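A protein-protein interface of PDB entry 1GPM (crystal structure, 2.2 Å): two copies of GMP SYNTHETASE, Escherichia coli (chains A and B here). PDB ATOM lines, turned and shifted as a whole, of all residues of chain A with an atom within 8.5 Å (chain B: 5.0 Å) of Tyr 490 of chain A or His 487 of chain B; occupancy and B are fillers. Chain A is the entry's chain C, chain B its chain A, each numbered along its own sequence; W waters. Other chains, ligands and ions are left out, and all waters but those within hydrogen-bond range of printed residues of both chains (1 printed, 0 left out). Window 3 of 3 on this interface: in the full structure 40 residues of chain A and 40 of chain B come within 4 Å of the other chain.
The backbone carbonyl oxygen of Leu 488 of chain B is in hydrogen-bond range of the side-chain hydroxyl of Tyr 490 of chain A (2.6 Å). The side-chain hydroxyl (OH) of Tyr 490 of chain B sits at hydrogen-bond distance from the backbone carbonyl oxygen (O) of Leu 488 of chain A (2.9 Å). The side-chain hydroxyl (OH) of Tyr 490 of chain A lies close to the backbone NH (N) of Tyr 490 of chain B (3.5 Å). N of Tyr 512 of chain A lies within hydrogen-bond range of O of Tyr 512 of chain B.
The backbone carbonyl oxygen (O) of Ala 486 of chain B lies within hydrogen-bond range of the side-chain hydroxyl (OH) of Tyr 512 of chain B (2.6 Å). The backbone carbonyl oxygen (O) of Ile 514 of chain A sits close to the indole nitrogen (NE1) of Trp 485 of chain A, 3.5 Å away. O of Gly 494 of chain A lies within hydrogen-bond range of OG of Ser 497 of chain A. The backbone carbonyl oxygen of Gly 494 of chain A lies within hydrogen-bond range of the side-chain amide nitrogen of Asn 498 of chain A (2.8 Å).
Tyr 490 of chain B touches Trp 485 of chain A. His 487 of chain A touches Tyr 490 of chain B (CE1 to CB, 3.4 Å). Tyr 490 of chain B touches Pro 489 of chain A. Tyr 490 of chain A touches Trp 485 of chain B. Tyr 490 of chain A touches His 487 of chain B (CB to ND1, 3.3 Å). Pro 489 of chain B touches Tyr 490 of chain A (CA to OH, 3.6 Å). Trp 485 of chain B touches Gly 494 of chain A (CZ2 to N, 3.8 Å).
Of the printed residues of chain B, Trp 485 of chain A touches Tyr 490. Tyr 490 of chain A touches five residues of chain B. No residue of chain A comes within 4 Å of Ala 486 of chain B. His 487 of chain B touches one residue of chain A. Printed residues of chain A within 4 Å of Leu 488 of chain B: Tyr 490 (2.6 Å). Printed residues of chain A within 4 Å of Pro 489 of chain B: Tyr 490. Printed residues of chain A within 4 Å of Tyr 512 of chain B: Tyr 512. The nearest residue of chain A that does not touch His 487 of chain B is Asp 491 of chain A (4.7 Å). The nearest printed residue of chain B that does not touch Tyr 512 of chain A is Tyr 490 of chain B (6.4 Å).
Printed residues of chain B that touch a printed residue of chain A: Trp 485, His 487, Leu 488, Pro 489, Tyr 490 and Tyr 512. Hydrophobic or aromatic side chains of chain B within 4 Å of the printed part of chain A: Trp 485, His 487, Tyr 490 and Tyr 512. Hydrophobic or aromatic side chains of chain A that line the printed part of chain B: Trp 485, His 487 and Tyr 490. Along chain A the printed residues that touch a printed residue of chain B span positions 485 to 512.
His 487 of chain A touches Tyr 490 of chain B, and with the chains exchanged Tyr 490 of chain A touches His 487 of chain B. Leu 488 of chain A touches Tyr 490 of chain B, and with the chains exchanged Tyr 490 of chain A touches Leu 488 of chain B. Pro 489 of chain A touches Tyr 490 of chain B, and with the chains exchanged Tyr 490 of chain A touches Pro 489 of chain B. Tyr 512 of chain A touches its own counterpart, Tyr 512 of chain B.
Water W1 lies within hydrogen-bond range of a ring nitrogen (NE2) of His 487 of chain A (2.7 Å) and the backbone carbonyl oxygen (O) of Tyr 490 of chain B (2.9 Å).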
ATOM      1  N   LEU A 440      18.867  14.370  -7.730  1.00  0.00           N
ATOM      2  CA  LEU A 440      18.010  14.157  -6.562  1.00  0.00           C
ATOM      3  C   LEU A 440      16.980  13.060  -6.794  1.00  0.00           C
ATOM      4  O   LEU A 440      16.466  12.466  -5.847  1.00  0.00           O
ATOM      5  CB  LEU A 440      17.294  15.442  -6.159  1.00  0.00           C
ATOM      6  CG  LEU A 440      18.109  16.492  -5.405  1.00  0.00           C
ATOM      7  CD1 LEU A 440      17.350  17.804  -5.394  1.00  0.00           C
ATOM      8  CD2 LEU A 440      18.396  16.015  -3.996  1.00  0.00           C
ATOM      9  N   TRP A 485       7.849  13.016   3.864  1.00  0.00           N
ATOM     10  CA  TRP A 485       7.809  14.013   2.794  1.00  0.00           C
ATOM     11  C   TRP A 485       9.264  14.458   2.714  1.00  0.00           C
ATOM     12  O   TRP A 485       9.924  14.622   3.745  1.00  0.00           O
ATOM     13  CB  TRP A 485       6.835  15.179   3.086  1.00  0.00           C
ATOM     14  CG  TRP A 485       7.110  16.023   4.314  1.00  0.00           C
ATOM     15  CD1 TRP A 485       6.609  15.826   5.571  1.00  0.00           C
ATOM     16  CD2 TRP A 485       7.923  17.202   4.390  1.00  0.00           C
ATOM     17  NE1 TRP A 485       7.064  16.804   6.423  1.00  0.00           N
ATOM     18  CE2 TRP A 485       7.874  17.664   5.725  1.00  0.00           C
ATOM     19  CE3 TRP A 485       8.694  17.915   3.460  1.00  0.00           C
ATOM     20  CZ2 TRP A 485       8.563  18.806   6.157  1.00  0.00           C
ATOM     21  CZ3 TRP A 485       9.379  19.049   3.890  1.00  0.00           C
ATOM     22  CH2 TRP A 485       9.311  19.481   5.222  1.00  0.00           C
ATOM     23  N   HIS A 487      12.737  16.405   2.335  1.00  0.00           N
ATOM     24  CA  HIS A 487      13.249  17.706   2.726  1.00  0.00           C
ATOM     25  C   HIS A 487      14.095  18.242   1.581  1.00  0.00           C
ATOM     26  O   HIS A 487      15.289  18.423   1.742  1.00  0.00           O
ATOM     27  CB  HIS A 487      14.097  17.604   4.014  1.00  0.00           C
ATOM     28  CG  HIS A 487      13.301  17.284   5.247  1.00  0.00           C
ATOM     29  ND1 HIS A 487      13.852  17.303   6.509  1.00  0.00           N
ATOM     30  CD2 HIS A 487      11.999  16.948   5.412  1.00  0.00           C
ATOM     31  CE1 HIS A 487      12.925  16.994   7.400  1.00  0.00           C
ATOM     32  NE2 HIS A 487      11.790  16.775   6.761  1.00  0.00           N
ATOM     33  N   LEU A 488      13.490  18.434   0.411  1.00  0.00           N
ATOM     34  CA  LEU A 488      14.207  18.962  -0.754  1.00  0.00           C
ATOM     35  C   LEU A 488      14.711  20.380  -0.460  1.00  0.00           C
ATOM     36  O   LEU A 488      14.006  21.178   0.168  1.00  0.00           O
ATOM     37  CB  LEU A 488      13.290  18.981  -1.981  1.00  0.00           C
ATOM     38  CG  LEU A 488      12.881  17.599  -2.492  1.00  0.00           C
ATOM     39  CD1 LEU A 488      11.850  17.720  -3.591  1.00  0.00           C
ATOM     40  CD2 LEU A 488      14.101  16.857  -2.990  1.00  0.00           C
ATOM     41  N   PRO A 489      15.939  20.709  -0.901  1.00  0.00           N
ATOM     42  CA  PRO A 489      16.537  22.032  -0.679  1.00  0.00           C
ATOM     43  C   PRO A 489      15.718  23.206  -1.196  1.00  0.00           C
ATOM     44  O   PRO A 489      15.278  23.217  -2.349  1.00  0.00           O
ATOM     45  CB  PRO A 489      17.896  21.923  -1.381  1.00  0.00           C
ATOM     46  CG  PRO A 489      17.699  20.850  -2.389  1.00  0.00           C
ATOM     47  CD  PRO A 489      16.870  19.841  -1.639  1.00  0.00           C
ATOM     48  N   TYR A 490      15.602  24.225  -0.346  1.00  0.00           N
ATOM     49  CA  TYR A 490      14.838  25.442  -0.626  1.00  0.00           C
ATOM     50  C   TYR A 490      15.103  26.103  -1.964  1.00  0.00           C
ATOM     51  O   TYR A 490      14.156  26.502  -2.653  1.00  0.00           O
ATOM     52  CB  TYR A 490      15.047  26.474   0.482  1.00  0.00           C
ATOM     53  CG  TYR A 490      14.669  25.983   1.861  1.00  0.00           C
ATOM     54  CD1 TYR A 490      13.337  25.914   2.260  1.00  0.00           C
ATOM     55  CD2 TYR A 490      15.650  25.579   2.765  1.00  0.00           C
ATOM     56  CE1 TYR A 490      12.991  25.452   3.523  1.00  0.00           C
ATOM     57  CE2 TYR A 490      15.315  25.122   4.024  1.00  0.00           C
ATOM     58  CZ  TYR A 490      13.984  25.060   4.398  1.00  0.00           C
ATOM     59  OH  TYR A 490      13.652  24.602   5.649  1.00  0.00           O
ATOM     60  N   ASP A 491      16.376  26.276  -2.317  1.00  0.00           N
ATOM     61  CA  ASP A 491      16.692  26.912  -3.592  1.00  0.00           C
ATOM     62  C   ASP A 491      16.294  26.024  -4.768  1.00  0.00           C
ATOM     63  O   ASP A 491      15.893  26.530  -5.814  1.00  0.00           O
ATOM     64  CB  ASP A 491      18.156  27.363  -3.671  1.00  0.00           C
ATOM     65  CG  ASP A 491      19.127  26.218  -3.566  1.00  0.00           C
ATOM     66  OD1 ASP A 491      19.333  25.714  -2.439  1.00  0.00           O
ATOM     67  OD2 ASP A 491      19.669  25.811  -4.619  1.00  0.00           O
ATOM     68  N   PHE A 492      16.378  24.706  -4.601  1.00  0.00           N
ATOM     69  CA  PHE A 492      15.957  23.792  -5.659  1.00  0.00           C
ATOM     70  C   PHE A 492      14.454  24.028  -5.862  1.00  0.00           C
ATOM     71  O   PHE A 492      13.987  24.184  -6.990  1.00  0.00           O
ATOM     72  CB  PHE A 492      16.220  22.330  -5.257  1.00  0.00           C
ATOM     73  CG  PHE A 492      15.496  21.317  -6.121  1.00  0.00           C
ATOM     74  CD1 PHE A 492      15.988  20.963  -7.375  1.00  0.00           C
ATOM     75  CD2 PHE A 492      14.296  20.748  -5.689  1.00  0.00           C
ATOM     76  CE1 PHE A 492      15.291  20.066  -8.183  1.00  0.00           C
ATOM     77  CE2 PHE A 492      13.597  19.854  -6.494  1.00  0.00           C
ATOM     78  CZ  PHE A 492      14.101  19.515  -7.746  1.00  0.00           C
ATOM     79  N   LEU A 493      13.724  24.117  -4.751  1.00  0.00           N
ATOM     80  CA  LEU A 493      12.277  24.347  -4.768  1.00  0.00           C
ATOM     81  C   LEU A 493      11.919  25.696  -5.404  1.00  0.00           C
ATOM     82  O   LEU A 493      11.029  25.766  -6.250  1.00  0.00           O
ATOM     83  CB  LEU A 493      11.693  24.247  -3.349  1.00  0.00           C
ATOM     84  CG  LEU A 493      11.673  22.850  -2.714  1.00  0.00           C
ATOM     85  CD1 LEU A 493      11.417  22.953  -1.217  1.00  0.00           C
ATOM     86  CD2 LEU A 493      10.622  21.977  -3.390  1.00  0.00           C
ATOM     87  N   GLY A 494      12.646  26.746  -5.031  1.00  0.00           N
ATOM     88  CA  GLY A 494      12.398  28.065  -5.590  1.00  0.00           C
ATOM     89  C   GLY A 494      12.618  28.072  -7.091  1.00  0.00           C
ATOM     90  O   GLY A 494      11.891  28.728  -7.844  1.00  0.00           O
ATOM     91  N   ARG A 495      13.638  27.335  -7.527  1.00  0.00           N
ATOM     92  CA  ARG A 495      13.977  27.211  -8.942  1.00  0.00           C
ATOM     93  C   ARG A 495      12.813  26.555  -9.694  1.00  0.00           C
ATOM     94  O   ARG A 495      12.301  27.092 -10.679  1.00  0.00           O
ATOM     95  CB  ARG A 495      15.231  26.351  -9.086  1.00  0.00           C
ATOM     96  CG  ARG A 495      15.823  26.286 -10.488  1.00  0.00           C
ATOM     97  CD  ARG A 495      17.076  25.408 -10.498  1.00  0.00           C
ATOM     98  NE  ARG A 495      17.923  25.681  -9.333  1.00  0.00           N
ATOM     99  CZ  ARG A 495      18.342  24.747  -8.479  1.00  0.00           C
ATOM    100  NH1 ARG A 495      17.997  23.469  -8.673  1.00  0.00           N
ATOM    101  NH2 ARG A 495      19.046  25.105  -7.398  1.00  0.00           N
ATOM    102  N   VAL A 496      12.368  25.416  -9.183  1.00  0.00           N
ATOM    103  CA  VAL A 496      11.272  24.688  -9.789  1.00  0.00           C
ATOM    104  C   VAL A 496       9.968  25.496  -9.870  1.00  0.00           C
ATOM    105  O   VAL A 496       9.349  25.564 -10.932  1.00  0.00           O
ATOM    106  CB  VAL A 496      11.041  23.347  -9.050  1.00  0.00           C
ATOM    107  CG1 VAL A 496       9.880  22.589  -9.670  1.00  0.00           C
ATOM    108  CG2 VAL A 496      12.311  22.501  -9.113  1.00  0.00           C
ATOM    109  N   SER A 497       9.553  26.128  -8.776  1.00  0.00           N
ATOM    110  CA  SER A 497       8.312  26.895  -8.810  1.00  0.00           C
ATOM    111  C   SER A 497       8.448  28.072  -9.751  1.00  0.00           C
ATOM    112  O   SER A 497       7.503  28.424 -10.468  1.00  0.00           O
ATOM    113  CB  SER A 497       7.879  27.352  -7.411  1.00  0.00           C
ATOM    114  OG  SER A 497       8.894  28.080  -6.749  1.00  0.00           O
ATOM    115  N   ASN A 498       9.642  28.653  -9.787  1.00  0.00           N
ATOM    116  CA  ASN A 498       9.901  29.780 -10.667  1.00  0.00           C
ATOM    117  C   ASN A 498       9.733  29.335 -12.114  1.00  0.00           C
ATOM    118  O   ASN A 498       8.907  29.889 -12.840  1.00  0.00           O
ATOM    119  CB  ASN A 498      11.309  30.339 -10.436  1.00  0.00           C
ATOM    120  CG  ASN A 498      11.366  31.322  -9.283  1.00  0.00           C
ATOM    121  OD1 ASN A 498      10.415  32.065  -9.043  1.00  0.00           O
ATOM    122  ND2 ASN A 498      12.479  31.327  -8.554  1.00  0.00           N
ATOM    123  N   TYR A 512       4.062  22.948  -2.181  1.00  0.00           N
ATOM    124  CA  TYR A 512       4.804  21.712  -1.962  1.00  0.00           C
ATOM    125  C   TYR A 512       4.178  20.949  -0.790  1.00  0.00           C
ATOM    126  O   TYR A 512       4.019  21.501   0.300  1.00  0.00           O
ATOM    127  CB  TYR A 512       6.274  22.021  -1.670  1.00  0.00           C
ATOM    128  CG  TYR A 512       7.087  20.785  -1.374  1.00  0.00           C
ATOM    129  CD1 TYR A 512       7.311  19.830  -2.358  1.00  0.00           C
ATOM    130  CD2 TYR A 512       7.559  20.529  -0.088  1.00  0.00           C
ATOM    131  CE1 TYR A 512       7.970  18.649  -2.068  1.00  0.00           C
ATOM    132  CE2 TYR A 512       8.221  19.350   0.212  1.00  0.00           C
ATOM    133  CZ  TYR A 512       8.418  18.415  -0.779  1.00  0.00           C
ATOM    134  OH  TYR A 512       9.022  17.224  -0.484  1.00  0.00           O
ATOM    135  N   ILE A 514       3.749  18.962   2.371  1.00  0.00           N
ATOM    136  CA  ILE A 514       4.550  18.696   3.562  1.00  0.00           C
ATOM    137  C   ILE A 514       3.805  17.757   4.506  1.00  0.00           C
ATOM    138  O   ILE A 514       3.869  17.901   5.715  1.00  0.00           O
ATOM    139  CB  ILE A 514       4.956  19.995   4.347  1.00  0.00           C
ATOM    140  CG1 ILE A 514       3.711  20.762   4.798  1.00  0.00           C
ATOM    141  CG2 ILE A 514       5.856  20.877   3.488  1.00  0.00           C
ATOM    142  CD1 ILE A 514       4.006  21.908   5.719  1.00  0.00           C
ATOM    143  N   GLU B 476       8.679  37.082   3.321  1.00  0.00           N
ATOM    144  CA  GLU B 476       9.546  38.147   3.798  1.00  0.00           C
ATOM    145  C   GLU B 476       9.393  39.218   2.729  1.00  0.00           C
ATOM    146  O   GLU B 476       9.867  39.068   1.600  1.00  0.00           O
ATOM    147  CB  GLU B 476      10.996  37.678   3.892  1.00  0.00           C
ATOM    148  CG  GLU B 476      11.250  36.774   5.074  1.00  0.00           C
ATOM    149  CD  GLU B 476      12.442  35.861   4.877  1.00  0.00           C
ATOM    150  OE1 GLU B 476      13.567  36.357   4.627  1.00  0.00           O
ATOM    151  OE2 GLU B 476      12.249  34.632   4.972  1.00  0.00           O
ATOM    152  N   TRP B 485       9.231  33.729  -0.374  1.00  0.00           N
ATOM    153  CA  TRP B 485       8.603  32.740   0.495  1.00  0.00           C
ATOM    154  C   TRP B 485       9.645  32.323   1.532  1.00  0.00           C
ATOM    155  O   TRP B 485      10.802  32.076   1.197  1.00  0.00           O
ATOM    156  CB  TRP B 485       8.034  31.544  -0.289  1.00  0.00           C
ATOM    157  CG  TRP B 485       9.004  30.751  -1.115  1.00  0.00           C
ATOM    158  CD1 TRP B 485       9.310  30.945  -2.431  1.00  0.00           C
ATOM    159  CD2 TRP B 485       9.763  29.609  -0.692  1.00  0.00           C
ATOM    160  NE1 TRP B 485      10.206  29.992  -2.857  1.00  0.00           N
ATOM    161  CE2 TRP B 485      10.507  29.163  -1.805  1.00  0.00           C
ATOM    162  CE3 TRP B 485       9.885  28.917   0.518  1.00  0.00           C
ATOM    163  CZ2 TRP B 485      11.364  28.063  -1.745  1.00  0.00           C
ATOM    164  CZ3 TRP B 485      10.738  27.816   0.577  1.00  0.00           C
ATOM    165  CH2 TRP B 485      11.464  27.404  -0.545  1.00  0.00           C
ATOM    166  N   ALA B 486       9.246  32.374   2.798  1.00  0.00           N
ATOM    167  CA  ALA B 486      10.102  32.033   3.933  1.00  0.00           C
ATOM    168  C   ALA B 486      10.620  30.593   3.932  1.00  0.00           C
ATOM    169  O   ALA B 486       9.857  29.634   3.788  1.00  0.00           O
ATOM    170  CB  ALA B 486       9.362  32.307   5.242  1.00  0.00           C
ATOM    171  N   HIS B 487      11.919  30.440   4.146  1.00  0.00           N
ATOM    172  CA  HIS B 487      12.523  29.117   4.177  1.00  0.00           C
ATOM    173  C   HIS B 487      12.374  28.545   5.578  1.00  0.00           C
ATOM    174  O   HIS B 487      13.368  28.368   6.285  1.00  0.00           O
ATOM    175  CB  HIS B 487      14.008  29.194   3.812  1.00  0.00           C
ATOM    176  CG  HIS B 487      14.269  29.576   2.391  1.00  0.00           C
ATOM    177  ND1 HIS B 487      15.517  29.479   1.816  1.00  0.00           N
ATOM    178  CD2 HIS B 487      13.447  30.052   1.427  1.00  0.00           C
ATOM    179  CE1 HIS B 487      15.453  29.878   0.558  1.00  0.00           C
ATOM    180  NE2 HIS B 487      14.208  30.231   0.296  1.00  0.00           N
ATOM    181  N   LEU B 488      11.143  28.260   5.987  1.00  0.00           N
ATOM    182  CA  LEU B 488      10.915  27.730   7.330  1.00  0.00           C
ATOM    183  C   LEU B 488      11.536  26.343   7.522  1.00  0.00           C
ATOM    184  O   LEU B 488      11.444  25.480   6.643  1.00  0.00           O
ATOM    185  CB  LEU B 488       9.427  27.714   7.655  1.00  0.00           C
ATOM    186  CG  LEU B 488       8.751  29.087   7.731  1.00  0.00           C
ATOM    187  CD1 LEU B 488       7.231  28.903   7.804  1.00  0.00           C
ATOM    188  CD2 LEU B 488       9.267  29.890   8.920  1.00  0.00           C
ATOM    189  N   PRO B 489      12.144  26.108   8.702  1.00  0.00           N
ATOM    190  CA  PRO B 489      12.808  24.860   9.093  1.00  0.00           C
ATOM    191  C   PRO B 489      11.905  23.648   8.928  1.00  0.00           C
ATOM    192  O   PRO B 489      10.806  23.610   9.477  1.00  0.00           O
ATOM    193  CB  PRO B 489      13.142  25.102  10.565  1.00  0.00           C
ATOM    194  CG  PRO B 489      13.278  26.595  10.651  1.00  0.00           C
ATOM    195  CD  PRO B 489      12.097  27.042   9.842  1.00  0.00           C
ATOM    196  N   TYR B 490      12.401  22.639   8.218  1.00  0.00           N
ATOM    197  CA  TYR B 490      11.640  21.421   7.945  1.00  0.00           C
ATOM    198  C   TYR B 490      10.997  20.779   9.177  1.00  0.00           C
ATOM    199  O   TYR B 490       9.854  20.332   9.115  1.00  0.00           O
ATOM    200  CB  TYR B 490      12.516  20.387   7.233  1.00  0.00           C
ATOM    201  CG  TYR B 490      13.240  20.881   5.987  1.00  0.00           C
ATOM    202  CD1 TYR B 490      12.609  20.899   4.737  1.00  0.00           C
ATOM    203  CD2 TYR B 490      14.575  21.283   6.052  1.00  0.00           C
ATOM    204  CE1 TYR B 490      13.293  21.298   3.587  1.00  0.00           C
ATOM    205  CE2 TYR B 490      15.264  21.683   4.914  1.00  0.00           C
ATOM    206  CZ  TYR B 490      14.621  21.687   3.689  1.00  0.00           C
ATOM    207  OH  TYR B 490      15.318  22.079   2.576  1.00  0.00           O
ATOM    208  N   TYR B 512       2.680  23.663   1.531  1.00  0.00           N
ATOM    209  CA  TYR B 512       3.359  24.919   1.788  1.00  0.00           C
ATOM    210  C   TYR B 512       3.558  25.710   0.501  1.00  0.00           C
ATOM    211  O   TYR B 512       3.987  25.150  -0.505  1.00  0.00           O
ATOM    212  CB  TYR B 512       4.704  24.659   2.461  1.00  0.00           C
ATOM    213  CG  TYR B 512       5.395  25.932   2.871  1.00  0.00           C
ATOM    214  CD1 TYR B 512       4.786  26.811   3.766  1.00  0.00           C
ATOM    215  CD2 TYR B 512       6.640  26.269   2.361  1.00  0.00           C
ATOM    216  CE1 TYR B 512       5.398  27.992   4.136  1.00  0.00           C
ATOM    217  CE2 TYR B 512       7.265  27.451   2.729  1.00  0.00           C
ATOM    218  CZ  TYR B 512       6.639  28.306   3.617  1.00  0.00           C
ATOM    219  OH  TYR B 512       7.246  29.475   4.005  1.00  0.00           O
HETATM  220  O   HOH W   1      10.499  17.510   9.062  1.00  0.00           O
